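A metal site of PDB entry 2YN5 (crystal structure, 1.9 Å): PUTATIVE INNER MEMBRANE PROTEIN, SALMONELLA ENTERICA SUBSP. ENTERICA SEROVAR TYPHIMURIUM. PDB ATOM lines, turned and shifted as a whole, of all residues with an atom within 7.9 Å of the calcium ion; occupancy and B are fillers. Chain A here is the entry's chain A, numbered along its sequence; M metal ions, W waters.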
ATOM      1  N   TYR A  56     -18.427  -0.608  15.387  1.00  0.00           N
ATOM      2  CA  TYR A  56     -18.869  -1.460  16.502  1.00  0.00           C
ATOM      3  C   TYR A  56     -20.394  -1.519  16.536  1.00  0.00           C
ATOM      4  O   TYR A  56     -21.043  -0.486  16.708  1.00  0.00           O
ATOM      5  CB  TYR A  56     -18.312  -0.931  17.813  1.00  0.00           C
ATOM      6  CG  TYR A  56     -18.594  -1.828  18.981  1.00  0.00           C
ATOM      7  CD1 TYR A  56     -17.722  -2.861  19.300  1.00  0.00           C
ATOM      8  CD2 TYR A  56     -19.725  -1.639  19.791  1.00  0.00           C
ATOM      9  CE1 TYR A  56     -17.979  -3.694  20.387  1.00  0.00           C
ATOM     10  CE2 TYR A  56     -19.980  -2.488  20.871  1.00  0.00           C
ATOM     11  CZ  TYR A  56     -19.093  -3.524  21.171  1.00  0.00           C
ATOM     12  OH  TYR A  56     -19.323  -4.385  22.242  1.00  0.00           O
ATOM     13  N   PRO A  57     -20.968  -2.718  16.347  1.00  0.00           N
ATOM     14  CA  PRO A  57     -22.421  -2.817  16.344  1.00  0.00           C
ATOM     15  C   PRO A  57     -23.017  -2.960  17.719  1.00  0.00           C
ATOM     16  O   PRO A  57     -22.370  -3.455  18.617  1.00  0.00           O
ATOM     17  CB  PRO A  57     -22.690  -4.104  15.562  1.00  0.00           C
ATOM     18  CG  PRO A  57     -21.461  -4.936  15.771  1.00  0.00           C
ATOM     19  CD  PRO A  57     -20.318  -4.004  16.053  1.00  0.00           C
ATOM     20  N   SER A  58     -24.285  -2.588  17.842  1.00  0.00           N
ATOM     21  CA  SER A  58     -25.025  -2.818  19.092  1.00  0.00           C
ATOM     22  C   SER A  58     -24.767  -4.219  19.671  1.00  0.00           C
ATOM     23  O   SER A  58     -24.906  -5.233  18.961  1.00  0.00           O
ATOM     24  CB  SER A  58     -26.523  -2.572  18.870  1.00  0.00           C
ATOM     25  OG  SER A  58     -27.296  -3.152  19.902  1.00  0.00           O
ATOM     26  N   GLU A  59     -24.361  -4.250  20.940  1.00  0.00           N
ATOM     27  CA  GLU A  59     -24.078  -5.460  21.728  1.00  0.00           C
ATOM     28  C   GLU A  59     -22.817  -6.234  21.272  1.00  0.00           C
ATOM     29  O   GLU A  59     -22.583  -7.341  21.755  1.00  0.00           O
ATOM     30  CB  GLU A  59     -25.298  -6.392  21.849  1.00  0.00           C
ATOM     31  CG  GLU A  59     -26.498  -5.671  22.481  1.00  0.00           C
ATOM     32  CD  GLU A  59     -27.769  -6.492  22.605  1.00  0.00           C
ATOM     33  OE1 GLU A  59     -27.854  -7.607  22.048  1.00  0.00           O
ATOM     34  OE2 GLU A  59     -28.710  -5.981  23.296  1.00  0.00           O
ATOM     35  N   GLY A  60     -22.008  -5.645  20.390  1.00  0.00           N
ATOM     36  CA  GLY A  60     -20.782  -6.315  19.894  1.00  0.00           C
ATOM     37  C   GLY A  60     -21.066  -7.563  19.052  1.00  0.00           C
ATOM     38  O   GLY A  60     -20.205  -8.453  18.928  1.00  0.00           O
ATOM     39  N   LYS A  61     -22.241  -7.613  18.434  1.00  0.00           N
ATOM     40  CA  LYS A  61     -22.728  -8.831  17.795  1.00  0.00           C
ATOM     41  C   LYS A  61     -22.692  -8.813  16.253  1.00  0.00           C
ATOM     42  O   LYS A  61     -23.276  -7.938  15.617  1.00  0.00           O
ATOM     43  CB  LYS A  61     -24.160  -9.116  18.226  1.00  0.00           C
ATOM     44  CG  LYS A  61     -24.326  -9.822  19.562  1.00  0.00           C
ATOM     45  CD  LYS A  61     -25.825  -9.931  19.801  1.00  0.00           C
ATOM     46  CE  LYS A  61     -26.129 -10.510  21.170  1.00  0.00           C
ATOM     47  NZ  LYS A  61     -27.551 -10.251  21.595  1.00  0.00           N
ATOM     48  N   LEU A  79     -19.661 -13.852  16.149  1.00  0.00           N
ATOM     49  CA  LEU A  79     -18.890 -13.173  17.182  1.00  0.00           C
ATOM     50  C   LEU A  79     -19.816 -12.351  18.057  1.00  0.00           C
ATOM     51  O   LEU A  79     -20.840 -11.841  17.580  1.00  0.00           O
ATOM     52  CB  LEU A  79     -17.791 -12.313  16.593  1.00  0.00           C
ATOM     53  CG  LEU A  79     -16.620 -13.191  16.087  1.00  0.00           C
ATOM     54  CD1 LEU A  79     -16.803 -13.513  14.603  1.00  0.00           C
ATOM     55  CD2 LEU A  79     -15.281 -12.534  16.333  1.00  0.00           C
ATOM     56  N   ASP A  80     -19.446 -12.239  19.331  1.00  0.00           N
ATOM     57  CA  ASP A  80     -20.206 -11.459  20.304  1.00  0.00           C
ATOM     58  C   ASP A  80     -19.155 -11.032  21.316  1.00  0.00           C
ATOM     59  O   ASP A  80     -18.683 -11.841  22.135  1.00  0.00           O
ATOM     60  CB  ASP A  80     -21.314 -12.276  20.940  1.00  0.00           C
ATOM     61  CG  ASP A  80     -22.185 -11.459  21.910  1.00  0.00           C
ATOM     62  OD1 ASP A  80     -21.758 -10.388  22.378  1.00  0.00           O
ATOM     63  OD2 ASP A  80     -23.292 -11.944  22.245  1.00  0.00           O
ATOM     64  N   ILE A  81     -18.710  -9.801  21.168  1.00  0.00           N
ATOM     65  CA  ILE A  81     -17.683  -9.203  22.017  1.00  0.00           C
ATOM     66  C   ILE A  81     -18.285  -8.116  22.932  1.00  0.00           C
ATOM     67  O   ILE A  81     -19.520  -7.920  22.955  1.00  0.00           O
ATOM     68  CB  ILE A  81     -16.515  -8.680  21.157  1.00  0.00           C
ATOM     69  CG1 ILE A  81     -16.967  -7.609  20.145  1.00  0.00           C
ATOM     70  CG2 ILE A  81     -15.874  -9.864  20.413  1.00  0.00           C
ATOM     71  CD1 ILE A  81     -15.785  -6.935  19.481  1.00  0.00           C
ATOM     72  N   MET A  82     -17.456  -7.453  23.727  1.00  0.00           N
ATOM     73  CA  MET A  82     -17.965  -6.382  24.596  1.00  0.00           C
ATOM     74  C   MET A  82     -16.859  -5.367  24.763  1.00  0.00           C
ATOM     75  O   MET A  82     -15.723  -5.719  25.054  1.00  0.00           O
ATOM     76  CB  MET A  82     -18.382  -6.931  25.967  1.00  0.00           C
ATOM     77  CG  MET A  82     -19.174  -5.943  26.837  1.00  0.00           C
ATOM     78  SD  MET A  82     -19.961  -6.680  28.296  1.00  0.00           S
ATOM     79  CE  MET A  82     -18.496  -7.096  29.233  1.00  0.00           C
ATOM     80  N   LYS A  83     -17.160  -4.092  24.551  1.00  0.00           N
ATOM     81  CA  LYS A  83     -16.067  -3.154  24.624  1.00  0.00           C
ATOM     82  C   LYS A  83     -16.083  -2.252  25.857  1.00  0.00           C
ATOM     83  O   LYS A  83     -15.036  -1.770  26.264  1.00  0.00           O
ATOM     84  CB  LYS A  83     -15.963  -2.328  23.343  1.00  0.00           C
ATOM     85  CG  LYS A  83     -17.002  -1.250  23.148  1.00  0.00           C
ATOM     86  CD  LYS A  83     -16.561  -0.319  22.023  1.00  0.00           C
ATOM     87  CE  LYS A  83     -17.639   0.670  21.644  1.00  0.00           C
ATOM     88  NZ  LYS A  83     -17.505   1.955  22.405  1.00  0.00           N
ATOM     89  N   GLU A 117     -23.413  -2.195  28.535  1.00  0.00           N
ATOM     90  CA  GLU A 117     -24.047  -2.452  27.267  1.00  0.00           C
ATOM     91  C   GLU A 117     -25.376  -3.173  27.454  1.00  0.00           C
ATOM     92  O   GLU A 117     -25.636  -3.763  28.506  1.00  0.00           O
ATOM     93  CB  GLU A 117     -23.072  -3.218  26.327  1.00  0.00           C
ATOM     94  CG  GLU A 117     -21.827  -2.399  25.970  1.00  0.00           C
ATOM     95  CD  GLU A 117     -20.908  -3.109  24.961  1.00  0.00           C
ATOM     96  OE1 GLU A 117     -21.430  -3.652  23.959  1.00  0.00           O
ATOM     97  OE2 GLU A 117     -19.666  -3.090  25.158  1.00  0.00           O
ATOM     98  N   SER A 118     -26.218  -3.139  26.421  1.00  0.00           N
ATOM     99  CA  SER A 118     -27.599  -3.588  26.562  1.00  0.00           C
ATOM    100  C   SER A 118     -27.727  -5.089  26.714  1.00  0.00           C
ATOM    101  O   SER A 118     -28.760  -5.564  27.177  1.00  0.00           O
ATOM    102  CB  SER A 118     -28.455  -3.067  25.402  1.00  0.00           C
ATOM    103  OG  SER A 118     -28.061  -3.659  24.169  1.00  0.00           O
ATOM    104  N   ASP A 119     -26.672  -5.842  26.367  1.00  0.00           N
ATOM    105  CA  ASP A 119     -26.743  -7.277  26.493  1.00  0.00           C
ATOM    106  C   ASP A 119     -26.140  -7.834  27.804  1.00  0.00           C
ATOM    107  O   ASP A 119     -25.982  -9.035  27.940  1.00  0.00           O
ATOM    108  CB  ASP A 119     -26.122  -7.953  25.256  1.00  0.00           C
ATOM    109  CG  ASP A 119     -24.644  -7.605  25.067  1.00  0.00           C
ATOM    110  OD1 ASP A 119     -24.216  -6.512  25.475  1.00  0.00           O
ATOM    111  OD2 ASP A 119     -23.912  -8.463  24.507  1.00  0.00           O
ATOM    112  N   VAL A 120     -25.850  -6.960  28.763  1.00  0.00           N
ATOM    113  CA  VAL A 120     -25.341  -7.349  30.075  1.00  0.00           C
ATOM    114  C   VAL A 120     -26.340  -8.261  30.817  1.00  0.00           C
ATOM    115  O   VAL A 120     -27.544  -7.950  30.907  1.00  0.00           O
ATOM    116  CB  VAL A 120     -24.924  -6.119  30.923  1.00  0.00           C
ATOM    117  CG1 VAL A 120     -24.533  -6.532  32.326  1.00  0.00           C
ATOM    118  CG2 VAL A 120     -23.720  -5.424  30.324  1.00  0.00           C
ATOM    119  N   SER A 162     -20.883  -8.669  32.834  1.00  0.00           N
ATOM    120  CA  SER A 162     -20.805  -9.738  31.828  1.00  0.00           C
ATOM    121  C   SER A 162     -22.016  -9.747  30.926  1.00  0.00           C
ATOM    122  O   SER A 162     -23.129  -9.530  31.392  1.00  0.00           O
ATOM    123  CB  SER A 162     -20.727 -11.104  32.507  1.00  0.00           C
ATOM    124  OG  SER A 162     -19.473 -11.282  33.097  1.00  0.00           O
ATOM    125  N   ASP A 163     -21.787  -9.984  29.639  1.00  0.00           N
ATOM    126  CA  ASP A 163     -22.913 -10.156  28.701  1.00  0.00           C
ATOM    127  C   ASP A 163     -23.357 -11.602  28.613  1.00  0.00           C
ATOM    128  O   ASP A 163     -22.733 -12.469  29.221  1.00  0.00           O
ATOM    129  CB  ASP A 163     -22.636  -9.538  27.305  1.00  0.00           C
ATOM    130  CG  ASP A 163     -21.483 -10.181  26.566  1.00  0.00           C
ATOM    131  OD1 ASP A 163     -20.946 -11.207  27.012  1.00  0.00           O
ATOM    132  OD2 ASP A 163     -21.097  -9.645  25.516  1.00  0.00           O
ATOM    133  N   ALA A 164     -24.420 -11.855  27.825  1.00  0.00           N
ATOM    134  CA  ALA A 164     -25.019 -13.180  27.634  1.00  0.00           C
ATOM    135  C   ALA A 164     -24.024 -14.158  27.026  1.00  0.00           C
ATOM    136  O   ALA A 164     -24.073 -15.358  27.293  1.00  0.00           O
ATOM    137  CB  ALA A 164     -26.293 -13.093  26.786  1.00  0.00           C
ATOM    138  N   ALA A 165     -23.111 -13.630  26.224  1.00  0.00           N
ATOM    139  CA  ALA A 165     -22.103 -14.445  25.535  1.00  0.00           C
ATOM    140  C   ALA A 165     -20.994 -14.877  26.473  1.00  0.00           C
ATOM    141  O   ALA A 165     -20.232 -15.792  26.169  1.00  0.00           O
ATOM    142  CB  ALA A 165     -21.528 -13.696  24.342  1.00  0.00           C
ATOM    143  N   GLY A 166     -20.875 -14.184  27.613  1.00  0.00           N
ATOM    144  CA  GLY A 166     -19.871 -14.552  28.595  1.00  0.00           C
ATOM    145  C   GLY A 166     -18.681 -13.612  28.673  1.00  0.00           C
ATOM    146  O   GLY A 166     -17.803 -13.840  29.477  1.00  0.00           O
ATOM    147  N   ASN A 167     -18.646 -12.564  27.851  1.00  0.00           N
ATOM    148  CA  ASN A 167     -17.583 -11.541  27.952  1.00  0.00           C
ATOM    149  C   ASN A 167     -17.677 -10.775  29.243  1.00  0.00           C
ATOM    150  O   ASN A 167     -18.776 -10.413  29.658  1.00  0.00           O
ATOM    151  CB  ASN A 167     -17.659 -10.519  26.821  1.00  0.00           C
ATOM    152  CG  ASN A 167     -17.668 -11.188  25.470  1.00  0.00           C
ATOM    153  OD1 ASN A 167     -16.685 -11.815  25.081  1.00  0.00           O
ATOM    154  ND2 ASN A 167     -18.793 -11.072  24.773  1.00  0.00           N
HETATM  155 CA    CA M   1     -21.681  -8.479  23.557  1.00  0.00          CA
HETATM  156  O   HOH W   1     -21.686  -6.250  24.736  1.00  0.00           O
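Water W1 lies within hydrogen-bond range of the side-chain carboxylate of Asp 119 (2.6 Å) and the side-chain carboxylate of Glu 117 (2.7 Å).
The backbone carbonyl oxygen (O) of Asp 80 sits at hydrogen-bond distance from the side-chain amide nitrogen (ND2) of Asn 167, 2.8 Å away. N of Ile 81 lies within hydrogen-bond range of O of Gly 60, 3.0 Å away. OE1 of Glu 59 lies within salt-bridge range of NZ of Lys 61 (2.7 Å). The side-chain carboxylate (OE2) of Glu 59 is in hydrogen-bond range of the side-chain hydroxyl (OG) of Ser 118, at 2.6 Å. OD1 of Asp 163 is in hydrogen-bond range of N of Asn 167. The side-chain carboxylate (OD1) of Asp 163 sits close to the backbone NH (N) of Ala 165 (3.3 Å). OD1 of Asp 163 sits at hydrogen-bond distance from N of Gly 166 (3.0 Å). The backbone carbonyl oxygen of Asp 119 is in hydrogen-bond range of the backbone NH of Ala 164 (3.2 Å).
The side-chain carboxylate (OD1) of Asp 80 binds the calcium ion. O of Ile 81 binds the calcium ion, at 2.3 Å. The calcium ion is bound by O of Glu 59, at 2.3 Å. The side-chain carboxylate (OD2) of Asp 163 binds the calcium ion (2.4 Å). The calcium ion is bound by the side-chain carboxylate (OD2) of Asp 119 (2.4 Å). Water W1 binds the calcium ion (2.5 Å). The calcium ion has six donor atoms within binding distance.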
